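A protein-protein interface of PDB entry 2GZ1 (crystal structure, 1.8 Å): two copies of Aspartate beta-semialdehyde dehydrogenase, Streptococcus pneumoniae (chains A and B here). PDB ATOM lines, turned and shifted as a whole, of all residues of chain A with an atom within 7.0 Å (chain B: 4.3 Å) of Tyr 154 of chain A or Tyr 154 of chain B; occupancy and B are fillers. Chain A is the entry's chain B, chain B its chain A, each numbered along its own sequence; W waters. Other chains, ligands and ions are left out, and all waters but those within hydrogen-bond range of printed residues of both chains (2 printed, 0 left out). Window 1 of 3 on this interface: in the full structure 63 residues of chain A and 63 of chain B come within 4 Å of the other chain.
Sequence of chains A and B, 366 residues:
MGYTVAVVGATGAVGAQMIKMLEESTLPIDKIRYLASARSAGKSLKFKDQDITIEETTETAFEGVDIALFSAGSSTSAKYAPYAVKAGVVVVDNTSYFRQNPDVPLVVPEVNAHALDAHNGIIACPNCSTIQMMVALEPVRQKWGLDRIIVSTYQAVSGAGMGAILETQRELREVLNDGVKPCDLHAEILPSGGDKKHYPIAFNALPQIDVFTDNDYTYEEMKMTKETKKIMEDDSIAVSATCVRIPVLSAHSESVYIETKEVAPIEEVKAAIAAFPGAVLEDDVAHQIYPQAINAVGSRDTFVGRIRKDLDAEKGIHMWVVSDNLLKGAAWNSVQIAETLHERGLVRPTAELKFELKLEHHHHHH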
ATOM      1  N   GLN A 132     -11.071 -41.044  -2.637  1.00  0.00           N
ATOM      2  CA  GLN A 132     -10.111 -40.596  -1.646  1.00  0.00           C
ATOM      3  C   GLN A 132     -10.768 -39.695  -0.593  1.00  0.00           C
ATOM      4  O   GLN A 132     -10.398 -39.742   0.570  1.00  0.00           O
ATOM      5  CB  GLN A 132      -8.900 -39.926  -2.305  1.00  0.00           C
ATOM      6  CG  GLN A 132      -9.155 -38.578  -2.933  1.00  0.00           C
ATOM      7  CD  GLN A 132      -7.932 -38.091  -3.674  1.00  0.00           C
ATOM      8  OE1 GLN A 132      -7.519 -38.703  -4.660  1.00  0.00           O
ATOM      9  NE2 GLN A 132      -7.347 -37.001  -3.203  1.00  0.00           N
ATOM     10  N   VAL A 151     -15.428 -28.912  -1.573  1.00  0.00           N
ATOM     11  CA  VAL A 151     -14.128 -29.414  -2.010  1.00  0.00           C
ATOM     12  C   VAL A 151     -13.631 -28.690  -3.267  1.00  0.00           C
ATOM     13  O   VAL A 151     -14.396 -28.419  -4.191  1.00  0.00           O
ATOM     14  CB  VAL A 151     -14.147 -30.964  -2.222  1.00  0.00           C
ATOM     15  CG1 VAL A 151     -15.221 -31.390  -3.178  1.00  0.00           C
ATOM     16  CG2 VAL A 151     -12.769 -31.484  -2.663  1.00  0.00           C
ATOM     17  N   SER A 152     -12.350 -28.374  -3.281  1.00  0.00           N
ATOM     18  CA  SER A 152     -11.676 -27.891  -4.483  1.00  0.00           C
ATOM     19  C   SER A 152     -10.536 -28.877  -4.767  1.00  0.00           C
ATOM     20  O   SER A 152      -9.713 -29.159  -3.893  1.00  0.00           O
ATOM     21  CB  SER A 152     -11.158 -26.469  -4.268  1.00  0.00           C
ATOM     22  OG  SER A 152     -12.242 -25.573  -4.057  1.00  0.00           O
ATOM     23  N   THR A 153     -10.515 -29.432  -5.972  1.00  0.00           N
ATOM     24  CA  THR A 153      -9.565 -30.470  -6.320  1.00  0.00           C
ATOM     25  C   THR A 153      -8.439 -29.960  -7.192  1.00  0.00           C
ATOM     26  O   THR A 153      -8.536 -28.916  -7.853  1.00  0.00           O
ATOM     27  CB  THR A 153     -10.239 -31.649  -7.056  1.00  0.00           C
ATOM     28  OG1 THR A 153     -10.544 -31.258  -8.399  1.00  0.00           O
ATOM     29  CG2 THR A 153     -11.587 -32.016  -6.442  1.00  0.00           C
ATOM     30  N   TYR A 154      -7.381 -30.764  -7.191  1.00  0.00           N
ATOM     31  CA  TYR A 154      -6.118 -30.471  -7.832  1.00  0.00           C
ATOM     32  C   TYR A 154      -5.768 -31.797  -8.498  1.00  0.00           C
ATOM     33  O   TYR A 154      -5.012 -32.607  -7.961  1.00  0.00           O
ATOM     34  CB  TYR A 154      -5.043 -30.095  -6.808  1.00  0.00           C
ATOM     35  CG  TYR A 154      -5.289 -28.831  -5.995  1.00  0.00           C
ATOM     36  CD1 TYR A 154      -4.458 -27.721  -6.124  1.00  0.00           C
ATOM     37  CD2 TYR A 154      -6.328 -28.769  -5.055  1.00  0.00           C
ATOM     38  CE1 TYR A 154      -4.672 -26.565  -5.375  1.00  0.00           C
ATOM     39  CE2 TYR A 154      -6.556 -27.615  -4.314  1.00  0.00           C
ATOM     40  CZ  TYR A 154      -5.734 -26.533  -4.455  1.00  0.00           C
ATOM     41  OH  TYR A 154      -5.985 -25.387  -3.725  1.00  0.00           O
ATOM     42  N   GLN A 155      -6.378 -32.036  -9.653  1.00  0.00           N
ATOM     43  CA  GLN A 155      -6.377 -33.368 -10.243  1.00  0.00           C
ATOM     44  C   GLN A 155      -5.308 -33.583 -11.316  1.00  0.00           C
ATOM     45  O   GLN A 155      -5.081 -32.736 -12.167  1.00  0.00           O
ATOM     46  CB  GLN A 155      -7.767 -33.707 -10.773  1.00  0.00           C
ATOM     47  CG  GLN A 155      -8.778 -33.958  -9.629  1.00  0.00           C
ATOM     48  CD  GLN A 155     -10.197 -34.192 -10.112  1.00  0.00           C
ATOM     49  OE1 GLN A 155     -11.116 -33.430  -9.767  1.00  0.00           O
ATOM     50  NE2 GLN A 155     -10.392 -35.259 -10.893  1.00  0.00           N
ATOM     51  N   ALA A 156      -4.674 -34.749 -11.240  1.00  0.00           N
ATOM     52  CA  ALA A 156      -3.625 -35.173 -12.156  1.00  0.00           C
ATOM     53  C   ALA A 156      -4.181 -35.560 -13.524  1.00  0.00           C
ATOM     54  O   ALA A 156      -5.308 -36.022 -13.636  1.00  0.00           O
ATOM     55  CB  ALA A 156      -2.879 -36.346 -11.567  1.00  0.00           C
ATOM     56  N   ALA A 205      -3.862 -24.192 -15.084  1.00  0.00           N
ATOM     57  CA  ALA A 205      -4.814 -24.822 -14.174  1.00  0.00           C
ATOM     58  C   ALA A 205      -6.188 -24.680 -14.813  1.00  0.00           C
ATOM     59  O   ALA A 205      -6.711 -23.579 -14.951  1.00  0.00           O
ATOM     60  CB  ALA A 205      -4.788 -24.153 -12.803  1.00  0.00           C
ATOM     61  N   ILE A 209     -13.204 -30.411 -15.612  1.00  0.00           N
ATOM     62  CA  ILE A 209     -13.017 -31.849 -15.724  1.00  0.00           C
ATOM     63  C   ILE A 209     -14.372 -32.419 -16.125  1.00  0.00           C
ATOM     64  O   ILE A 209     -15.413 -32.101 -15.517  1.00  0.00           O
ATOM     65  CB  ILE A 209     -12.496 -32.433 -14.387  1.00  0.00           C
ATOM     66  CG1 ILE A 209     -11.124 -31.798 -14.068  1.00  0.00           C
ATOM     67  CG2 ILE A 209     -12.450 -33.952 -14.458  1.00  0.00           C
ATOM     68  CD1 ILE A 209     -10.344 -32.439 -13.003  1.00  0.00           C
ATOM     69  N   THR A 242     -15.531 -27.893  -6.784  1.00  0.00           N
ATOM     70  CA  THR A 242     -14.844 -27.278  -7.912  1.00  0.00           C
ATOM     71  C   THR A 242     -13.688 -28.215  -8.294  1.00  0.00           C
ATOM     72  O   THR A 242     -12.793 -28.491  -7.476  1.00  0.00           O
ATOM     73  CB  THR A 242     -14.300 -25.892  -7.549  1.00  0.00           C
ATOM     74  OG1 THR A 242     -15.351 -25.016  -7.115  1.00  0.00           O
ATOM     75  CG2 THR A 242     -13.755 -25.203  -8.772  1.00  0.00           C
ATOM     76  N   CYS A 243     -13.699 -28.687  -9.533  1.00  0.00           N
ATOM     77  CA  CYS A 243     -12.744 -29.679  -9.995  1.00  0.00           C
ATOM     78  C   CYS A 243     -11.810 -29.091 -11.042  1.00  0.00           C
ATOM     79  O   CYS A 243     -12.251 -28.606 -12.085  1.00  0.00           O
ATOM     80  CB  CYS A 243     -13.471 -30.913 -10.522  1.00  0.00           C
ATOM     81  SG  CYS A 243     -14.414 -31.738  -9.218  1.00  0.00           S
ATOM     82  N   VAL A 244     -10.521 -29.121 -10.737  1.00  0.00           N
ATOM     83  CA  VAL A 244      -9.512 -28.423 -11.524  1.00  0.00           C
ATOM     84  C   VAL A 244      -8.394 -29.376 -11.889  1.00  0.00           C
ATOM     85  O   VAL A 244      -7.844 -30.070 -11.022  1.00  0.00           O
ATOM     86  CB  VAL A 244      -8.913 -27.237 -10.725  1.00  0.00           C
ATOM     87  CG1 VAL A 244      -7.917 -26.452 -11.544  1.00  0.00           C
ATOM     88  CG2 VAL A 244     -10.041 -26.330 -10.164  1.00  0.00           C
ATOM     89  N   ARG A 245      -8.051 -29.397 -13.172  1.00  0.00           N
ATOM     90  CA  ARG A 245      -6.889 -30.118 -13.654  1.00  0.00           C
ATOM     91  C   ARG A 245      -5.624 -29.266 -13.527  1.00  0.00           C
ATOM     92  O   ARG A 245      -5.607 -28.111 -13.960  1.00  0.00           O
ATOM     93  CB  ARG A 245      -7.086 -30.500 -15.123  1.00  0.00           C
ATOM     94  CG  ARG A 245      -6.126 -31.561 -15.590  1.00  0.00           C
ATOM     95  CD  ARG A 245      -6.521 -32.947 -15.165  1.00  0.00           C
ATOM     96  NE  ARG A 245      -7.746 -33.368 -15.833  1.00  0.00           N
ATOM     97  CZ  ARG A 245      -8.400 -34.476 -15.560  1.00  0.00           C
ATOM     98  NH1 ARG A 245      -7.947 -35.325 -14.648  1.00  0.00           N
ATOM     99  NH2 ARG A 245      -9.516 -34.748 -16.219  1.00  0.00           N
ATOM    100  N   ILE A 246      -4.571 -29.836 -12.952  1.00  0.00           N
ATOM    101  CA  ILE A 246      -3.274 -29.173 -12.876  1.00  0.00           C
ATOM    102  C   ILE A 246      -2.178 -30.049 -13.490  1.00  0.00           C
ATOM    103  O   ILE A 246      -2.424 -31.221 -13.743  1.00  0.00           O
ATOM    104  CB  ILE A 246      -2.934 -28.807 -11.403  1.00  0.00           C
ATOM    105  CG1 ILE A 246      -2.814 -30.064 -10.536  1.00  0.00           C
ATOM    106  CG2 ILE A 246      -3.977 -27.852 -10.821  1.00  0.00           C
ATOM    107  CD1 ILE A 246      -2.135 -29.811  -9.213  1.00  0.00           C
ATOM    108  N   VAL A 248       0.148 -32.224 -13.022  1.00  0.00           N
ATOM    109  CA  VAL A 248       0.653 -33.349 -12.225  1.00  0.00           C
ATOM    110  C   VAL A 248       0.285 -34.582 -13.043  1.00  0.00           C
ATOM    111  O   VAL A 248      -0.810 -34.654 -13.591  1.00  0.00           O
ATOM    112  CB  VAL A 248      -0.023 -33.367 -10.820  1.00  0.00           C
ATOM    113  CG1 VAL A 248       0.278 -34.665 -10.038  1.00  0.00           C
ATOM    114  CG2 VAL A 248       0.402 -32.128 -10.027  1.00  0.00           C
ATOM    115  N   ALA A 251      -1.689 -38.739  -9.112  1.00  0.00           N
ATOM    116  CA  ALA A 251      -2.118 -38.431  -7.756  1.00  0.00           C
ATOM    117  C   ALA A 251      -2.927 -37.146  -7.705  1.00  0.00           C
ATOM    118  O   ALA A 251      -2.438 -36.088  -8.081  1.00  0.00           O
ATOM    119  CB  ALA A 251      -0.958 -38.389  -6.760  1.00  0.00           C
ATOM    120  N   HIS A 252      -4.176 -37.276  -7.263  1.00  0.00           N
ATOM    121  CA  HIS A 252      -5.064 -36.155  -7.042  1.00  0.00           C
ATOM    122  C   HIS A 252      -4.849 -35.620  -5.633  1.00  0.00           C
ATOM    123  O   HIS A 252      -4.626 -36.385  -4.684  1.00  0.00           O
ATOM    124  CB  HIS A 252      -6.518 -36.593  -7.153  1.00  0.00           C
ATOM    125  CG  HIS A 252      -6.942 -37.034  -8.527  1.00  0.00           C
ATOM    126  ND1 HIS A 252      -6.243 -36.729  -9.675  1.00  0.00           N
ATOM    127  CD2 HIS A 252      -8.024 -37.746  -8.927  1.00  0.00           C
ATOM    128  CE1 HIS A 252      -6.877 -37.227 -10.723  1.00  0.00           C
ATOM    129  NE2 HIS A 252      -7.963 -37.851 -10.297  1.00  0.00           N
ATOM    130  N   SER A 253      -4.938 -34.305  -5.492  1.00  0.00           N
ATOM    131  CA  SER A 253      -4.985 -33.664  -4.192  1.00  0.00           C
ATOM    132  C   SER A 253      -6.287 -32.887  -4.042  1.00  0.00           C
ATOM    133  O   SER A 253      -6.865 -32.423  -5.027  1.00  0.00           O
ATOM    134  CB  SER A 253      -3.802 -32.704  -4.012  1.00  0.00           C
ATOM    135  OG  SER A 253      -2.599 -33.245  -4.508  1.00  0.00           O
ATOM    136  N   GLU A 254      -6.767 -32.753  -2.816  1.00  0.00           N
ATOM    137  CA  GLU A 254      -8.018 -32.043  -2.562  1.00  0.00           C
ATOM    138  C   GLU A 254      -7.927 -31.162  -1.326  1.00  0.00           C
ATOM    139  O   GLU A 254      -7.457 -31.600  -0.274  1.00  0.00           O
ATOM    140  CB  GLU A 254      -9.173 -33.036  -2.392  1.00  0.00           C
ATOM    141  CG  GLU A 254      -9.431 -33.916  -3.595  1.00  0.00           C
ATOM    142  CD  GLU A 254     -10.316 -35.102  -3.298  1.00  0.00           C
ATOM    143  OE1 GLU A 254     -10.383 -35.569  -2.134  1.00  0.00           O
ATOM    144  OE2 GLU A 254     -10.919 -35.597  -4.259  1.00  0.00           O
ATOM    145  N   SER A 255      -8.365 -29.915  -1.460  1.00  0.00           N
ATOM    146  CA  SER A 255      -8.656 -29.062  -0.317  1.00  0.00           C
ATOM    147  C   SER A 255     -10.115 -29.278   0.074  1.00  0.00           C
ATOM    148  O   SER A 255     -11.027 -28.913  -0.662  1.00  0.00           O
ATOM    149  CB  SER A 255      -8.399 -27.587  -0.636  1.00  0.00           C
ATOM    150  OG  SER A 255      -8.783 -26.749   0.448  1.00  0.00           O
ATOM    151  N   ALA A 293       1.304 -35.133  -3.645  1.00  0.00           N
ATOM    152  CA  ALA A 293       1.109 -35.971  -4.840  1.00  0.00           C
ATOM    153  C   ALA A 293       2.326 -36.845  -5.146  1.00  0.00           C
ATOM    154  O   ALA A 293       2.195 -38.051  -5.333  1.00  0.00           O
ATOM    155  CB  ALA A 293       0.792 -35.100  -6.039  1.00  0.00           C
ATOM    156  N   TRP A 320      -6.328 -31.590   3.750  1.00  0.00           N
ATOM    157  CA  TRP A 320      -5.674 -31.816   2.461  1.00  0.00           C
ATOM    158  C   TRP A 320      -5.596 -33.328   2.301  1.00  0.00           C
ATOM    159  O   TRP A 320      -5.039 -34.017   3.149  1.00  0.00           O
ATOM    160  CB  TRP A 320      -4.282 -31.198   2.507  1.00  0.00           C
ATOM    161  CG  TRP A 320      -3.442 -31.261   1.247  1.00  0.00           C
ATOM    162  CD1 TRP A 320      -2.277 -31.952   1.063  1.00  0.00           C
ATOM    163  CD2 TRP A 320      -3.682 -30.562   0.033  1.00  0.00           C
ATOM    164  NE1 TRP A 320      -1.778 -31.724  -0.196  1.00  0.00           N
ATOM    165  CE2 TRP A 320      -2.623 -30.878  -0.856  1.00  0.00           C
ATOM    166  CE3 TRP A 320      -4.686 -29.690  -0.406  1.00  0.00           C
ATOM    167  CZ2 TRP A 320      -2.546 -30.364  -2.141  1.00  0.00           C
ATOM    168  CZ3 TRP A 320      -4.606 -29.184  -1.689  1.00  0.00           C
ATOM    169  CH2 TRP A 320      -3.537 -29.528  -2.545  1.00  0.00           C
ATOM    170  N   SER B 152      -9.452 -21.672  -1.707  1.00  0.00           N
ATOM    171  CA  SER B 152      -8.336 -22.584  -1.939  1.00  0.00           C
ATOM    172  C   SER B 152      -7.557 -22.050  -3.117  1.00  0.00           C
ATOM    173  O   SER B 152      -8.120 -21.805  -4.182  1.00  0.00           O
ATOM    174  CB  SER B 152      -8.837 -23.994  -2.222  1.00  0.00           C
ATOM    175  OG  SER B 152      -9.519 -24.535  -1.106  1.00  0.00           O
ATOM    176  N   THR B 153      -6.255 -21.834  -2.932  1.00  0.00           N
ATOM    177  CA  THR B 153      -5.461 -21.216  -3.972  1.00  0.00           C
ATOM    178  C   THR B 153      -4.591 -22.223  -4.724  1.00  0.00           C
ATOM    179  O   THR B 153      -4.288 -23.322  -4.242  1.00  0.00           O
ATOM    180  CB  THR B 153      -4.565 -20.074  -3.448  1.00  0.00           C
ATOM    181  OG1 THR B 153      -3.452 -20.610  -2.726  1.00  0.00           O
ATOM    182  CG2 THR B 153      -5.280 -19.160  -2.436  1.00  0.00           C
ATOM    183  N   TYR B 154      -4.177 -21.764  -5.895  1.00  0.00           N
ATOM    184  CA  TYR B 154      -3.447 -22.531  -6.894  1.00  0.00           C
ATOM    185  C   TYR B 154      -2.359 -21.571  -7.375  1.00  0.00           C
ATOM    186  O   TYR B 154      -2.479 -20.930  -8.423  1.00  0.00           O
ATOM    187  CB  TYR B 154      -4.379 -22.913  -8.044  1.00  0.00           C
ATOM    188  CG  TYR B 154      -5.528 -23.841  -7.707  1.00  0.00           C
ATOM    189  CD1 TYR B 154      -5.585 -25.127  -8.236  1.00  0.00           C
ATOM    190  CD2 TYR B 154      -6.587 -23.423  -6.890  1.00  0.00           C
ATOM    191  CE1 TYR B 154      -6.653 -25.968  -7.956  1.00  0.00           C
ATOM    192  CE2 TYR B 154      -7.659 -24.245  -6.622  1.00  0.00           C
ATOM    193  CZ  TYR B 154      -7.676 -25.530  -7.130  1.00  0.00           C
ATOM    194  OH  TYR B 154      -8.725 -26.369  -6.866  1.00  0.00           O
ATOM    195  N   GLN B 155      -1.304 -21.439  -6.588  1.00  0.00           N
ATOM    196  CA  GLN B 155      -0.379 -20.325  -6.744  1.00  0.00           C
ATOM    197  C   GLN B 155       0.868 -20.683  -7.537  1.00  0.00           C
ATOM    198  O   GLN B 155       1.461 -21.731  -7.343  1.00  0.00           O
ATOM    199  CB  GLN B 155      -0.013 -19.732  -5.375  1.00  0.00           C
ATOM    200  CG  GLN B 155      -1.188 -18.948  -4.750  1.00  0.00           C
ATOM    201  CD  GLN B 155      -0.898 -18.389  -3.364  1.00  0.00           C
ATOM    202  OE1 GLN B 155      -1.621 -18.692  -2.414  1.00  0.00           O
ATOM    203  NE2 GLN B 155       0.163 -17.580  -3.240  1.00  0.00           N
ATOM    204  N   ALA B 156       1.234 -19.775  -8.434  1.00  0.00           N
ATOM    205  CA  ALA B 156       2.397 -19.907  -9.289  1.00  0.00           C
ATOM    206  C   ALA B 156       3.716 -19.721  -8.545  1.00  0.00           C
ATOM    207  O   ALA B 156       3.782 -19.032  -7.549  1.00  0.00           O
ATOM    208  CB  ALA B 156       2.296 -18.905 -10.425  1.00  0.00           C
ATOM    209  N   VAL B 244      -1.893 -23.174  -1.775  1.00  0.00           N
ATOM    210  CA  VAL B 244      -1.174 -24.292  -2.387  1.00  0.00           C
ATOM    211  C   VAL B 244      -0.330 -23.796  -3.553  1.00  0.00           C
ATOM    212  O   VAL B 244      -0.823 -23.044  -4.406  1.00  0.00           O
ATOM    213  CB  VAL B 244      -2.176 -25.369  -2.877  1.00  0.00           C
ATOM    214  CG1 VAL B 244      -1.472 -26.599  -3.455  1.00  0.00           C
ATOM    215  CG2 VAL B 244      -3.100 -25.790  -1.741  1.00  0.00           C
ATOM    216  N   ILE B 246       1.422 -24.770  -7.002  1.00  0.00           N
ATOM    217  CA  ILE B 246       1.379 -25.743  -8.084  1.00  0.00           C
ATOM    218  C   ILE B 246       2.410 -25.400  -9.171  1.00  0.00           C
ATOM    219  O   ILE B 246       2.944 -24.291  -9.168  1.00  0.00           O
ATOM    220  CB  ILE B 246      -0.053 -25.831  -8.654  1.00  0.00           C
ATOM    221  CG1 ILE B 246      -0.526 -24.497  -9.255  1.00  0.00           C
ATOM    222  CG2 ILE B 246      -0.999 -26.286  -7.571  1.00  0.00           C
ATOM    223  CD1 ILE B 246      -1.682 -24.663 -10.215  1.00  0.00           C
ATOM    224  N   HIS B 252      -1.727 -16.607 -10.448  1.00  0.00           N
ATOM    225  CA  HIS B 252      -2.416 -17.359  -9.412  1.00  0.00           C
ATOM    226  C   HIS B 252      -3.870 -17.595  -9.814  1.00  0.00           C
ATOM    227  O   HIS B 252      -4.484 -16.742 -10.437  1.00  0.00           O
ATOM    228  CB  HIS B 252      -2.409 -16.575  -8.104  1.00  0.00           C
ATOM    229  CG  HIS B 252      -1.049 -16.381  -7.497  1.00  0.00           C
ATOM    230  ND1 HIS B 252       0.020 -17.209  -7.750  1.00  0.00           N
ATOM    231  CD2 HIS B 252      -0.598 -15.446  -6.628  1.00  0.00           C
ATOM    232  CE1 HIS B 252       1.067 -16.803  -7.057  1.00  0.00           C
ATOM    233  NE2 HIS B 252       0.716 -15.740  -6.359  1.00  0.00           N
ATOM    234  N   SER B 253      -4.412 -18.749  -9.426  1.00  0.00           N
ATOM    235  CA  SER B 253      -5.814 -19.088  -9.593  1.00  0.00           C
ATOM    236  C   SER B 253      -6.396 -19.400  -8.225  1.00  0.00           C
ATOM    237  O   SER B 253      -5.675 -19.879  -7.345  1.00  0.00           O
ATOM    238  CB  SER B 253      -5.983 -20.308 -10.500  1.00  0.00           C
ATOM    239  OG  SER B 253      -5.222 -20.191 -11.679  1.00  0.00           O
ATOM    240  N   SER B 255     -10.056 -20.947  -6.196  1.00  0.00           N
ATOM    241  CA  SER B 255     -11.418 -21.412  -6.048  1.00  0.00           C
ATOM    242  C   SER B 255     -11.964 -20.689  -4.819  1.00  0.00           C
ATOM    243  O   SER B 255     -11.480 -20.888  -3.694  1.00  0.00           O
ATOM    244  CB  SER B 255     -11.466 -22.929  -5.882  1.00  0.00           C
ATOM    245  OG  SER B 255     -12.778 -23.395  -5.620  1.00  0.00           O
ATOM    246  N   TRP B 320     -14.173 -18.743  -9.763  1.00  0.00           N
ATOM    247  CA  TRP B 320     -12.794 -19.043 -10.095  1.00  0.00           C
ATOM    248  C   TRP B 320     -12.140 -17.726 -10.512  1.00  0.00           C
ATOM    249  O   TRP B 320     -12.610 -17.070 -11.433  1.00  0.00           O
ATOM    250  CB  TRP B 320     -12.767 -20.023 -11.253  1.00  0.00           C
ATOM    251  CG  TRP B 320     -11.405 -20.480 -11.729  1.00  0.00           C
ATOM    252  CD1 TRP B 320     -10.830 -20.215 -12.956  1.00  0.00           C
ATOM    253  CD2 TRP B 320     -10.484 -21.345 -11.046  1.00  0.00           C
ATOM    254  NE1 TRP B 320      -9.614 -20.834 -13.053  1.00  0.00           N
ATOM    255  CE2 TRP B 320      -9.370 -21.532 -11.900  1.00  0.00           C
ATOM    256  CE3 TRP B 320     -10.475 -21.965  -9.793  1.00  0.00           C
ATOM    257  CZ2 TRP B 320      -8.272 -22.318 -11.545  1.00  0.00           C
ATOM    258  CZ3 TRP B 320      -9.398 -22.740  -9.438  1.00  0.00           C
ATOM    259  CH2 TRP B 320      -8.300 -22.915 -10.315  1.00  0.00           C
HETATM  260  O   HOH W   1     -12.084 -24.755  -1.562  1.00  0.00           O
HETATM  261  O   HOH W   2      -6.239 -21.030 -14.141  1.00  0.00           O
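Among the printed residues, pairs that only touch across the chains: Tyr 154 of chain A with Tyr 154 of chain B, Tyr 154 of chain A with Ser 152 of chain B, Tyr 154 of chain A with Val 244 of chain B, Val 244 of chain A with Tyr 154 of chain B, Ser 152 of chain A with Tyr 154 of chain B, Trp 320 of chain A with Val 244 of chain B, Val 244 of chain A with Trp 320 of chain B, Ala 205 of chain A with Trp 320 of chain B, Ser 152 of chain A with Ser 152 of chain B and Ile 246 of chain A with Ile 246 of chain B.
Printed residues of chain B within 4 Å of Tyr 154 of chain A: Ser 152, Thr 153, Tyr 154 and Val 244. Of chain A, only Ser 152 (3.6 Å), Thr 153 (2.7 Å), Tyr 154 (3.3 Å) and Val 244 (3.6 Å) come within 4 Å of Tyr 154 of chain B. Of the printed residues of chain B, Trp 320 of chain A touches Val 244 (3.7 Å). Printed residues of chain A within 4 Å of Ser 255 of chain B: Ser 152 (2.7 Å) and Thr 242 (3.4 Å). Of the printed residues of chain A, Ser 152 of chain B touches Ser 152, Tyr 154 and Ser 255. Ile 209 of chain A touches none of the printed residues of chain B. Ala 156 of chain A touches none of the printed residues of chain B. The nearest printed residue of chain B that does not touch Tyr 154 of chain A is Ile 246 of chain B (4.01 Å). The nearest printed residue of chain A that does not touch Ser 152 of chain B is Val 151 of chain A (6.2 Å).
Ser 152 of chain A touches Tyr 154 of chain B, and with the chains exchanged Tyr 154 of chain A touches Ser 152 of chain B. Ser 152 of chain A touches Ser 255 of chain B, and with the chains exchanged Ser 255 of chain A touches Ser 152 of chain B. Tyr 154 of chain A touches Val 244 of chain B, and with the chains exchanged Val 244 of chain A touches Tyr 154 of chain B. Ile 246 of chain A touches its own counterpart, Ile 246 of chain B. Positions printed for both chains: 152, 153, 154, 155, 156, 244, 246, 252, 253, 255 and 320. Of the 15 pairs that touch across the chains among the printed residues, 13 have their exchanged pair printed and touching as well.
The side-chain hydroxyl (OH) of Tyr 154 of chain B lies within hydrogen-bond range of the backbone carbonyl oxygen (O) of Thr 153 of chain A, at 2.7 Å. The backbone carbonyl oxygen of Thr 153 of chain B sits at hydrogen-bond distance from the side-chain hydroxyl of Tyr 154 of chain A (2.7 Å). The side-chain hydroxyl of Ser 152 of chain B lies within hydrogen-bond range of the side-chain hydroxyl of Ser 255 of chain A, at 2.8 Å. The side-chain hydroxyl (OG) of Ser 255 of chain B sits at hydrogen-bond distance from the side-chain hydroxyl (OG1) of Thr 242 of chain A (3.4 Å). The side-chain hydroxyl of Ser 255 of chain B lies within hydrogen-bond range of the side-chain hydroxyl of Ser 152 of chain A (2.7 Å).
Of the 11 printed residues of chain B, 7 touch a printed residue of chain A. Hydrophobic or aromatic side chains of chain B that line the printed part of chain A: Tyr 154, Val 244, Ile 246 and Trp 320. Printed residues of chain A that touch a printed residue of chain B: Ser 152, Thr 153, Tyr 154, Ala 205, Thr 242, Val 244, Ile 246, Ser 255 and Trp 320. Among the printed residues, 15 pairs touch across the chains. Among the printed residues, no Asp or Glu carboxylate lies within 4 Å of a Lys or Arg side-chain nitrogen of the other chain.
N of Gln 155 of chain A lies within hydrogen-bond range of O of Val 244 of chain A, 2.8 Å away. The side-chain hydroxyl of Thr 153 of chain B lies within hydrogen-bond range of the side-chain amide oxygen of Gln 155 of chain B, at 2.7 Å. The backbone carbonyl oxygen (O) of Ser 152 of chain B is in hydrogen-bond range of the backbone NH (N) of Ser 255 of chain B (2.9 Å). The side-chain hydroxyl (OG1) of Thr 153 of chain B is in hydrogen-bond range of the backbone NH (N) of Val 244 of chain B, 3.1 Å away. The side-chain hydroxyl of Thr 153 of chain A lies within hydrogen-bond range of the side-chain amide oxygen of Gln 155 of chain A, at 2.6 Å. O of Gln 155 of chain B sits at hydrogen-bond distance from N of Ile 246 of chain B.
Water W1 bridges OG of Ser 152 of chain B (2.6 Å) and OG of Ser 152 of chain A (2.6 Å). Water W2 lies within hydrogen-bond range of the backbone carbonyl oxygen (O) of Ala 205 of chain A (2.7 Å) and the side-chain hydroxyl (OG) of Ser 253 of chain B (2.8 Å).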
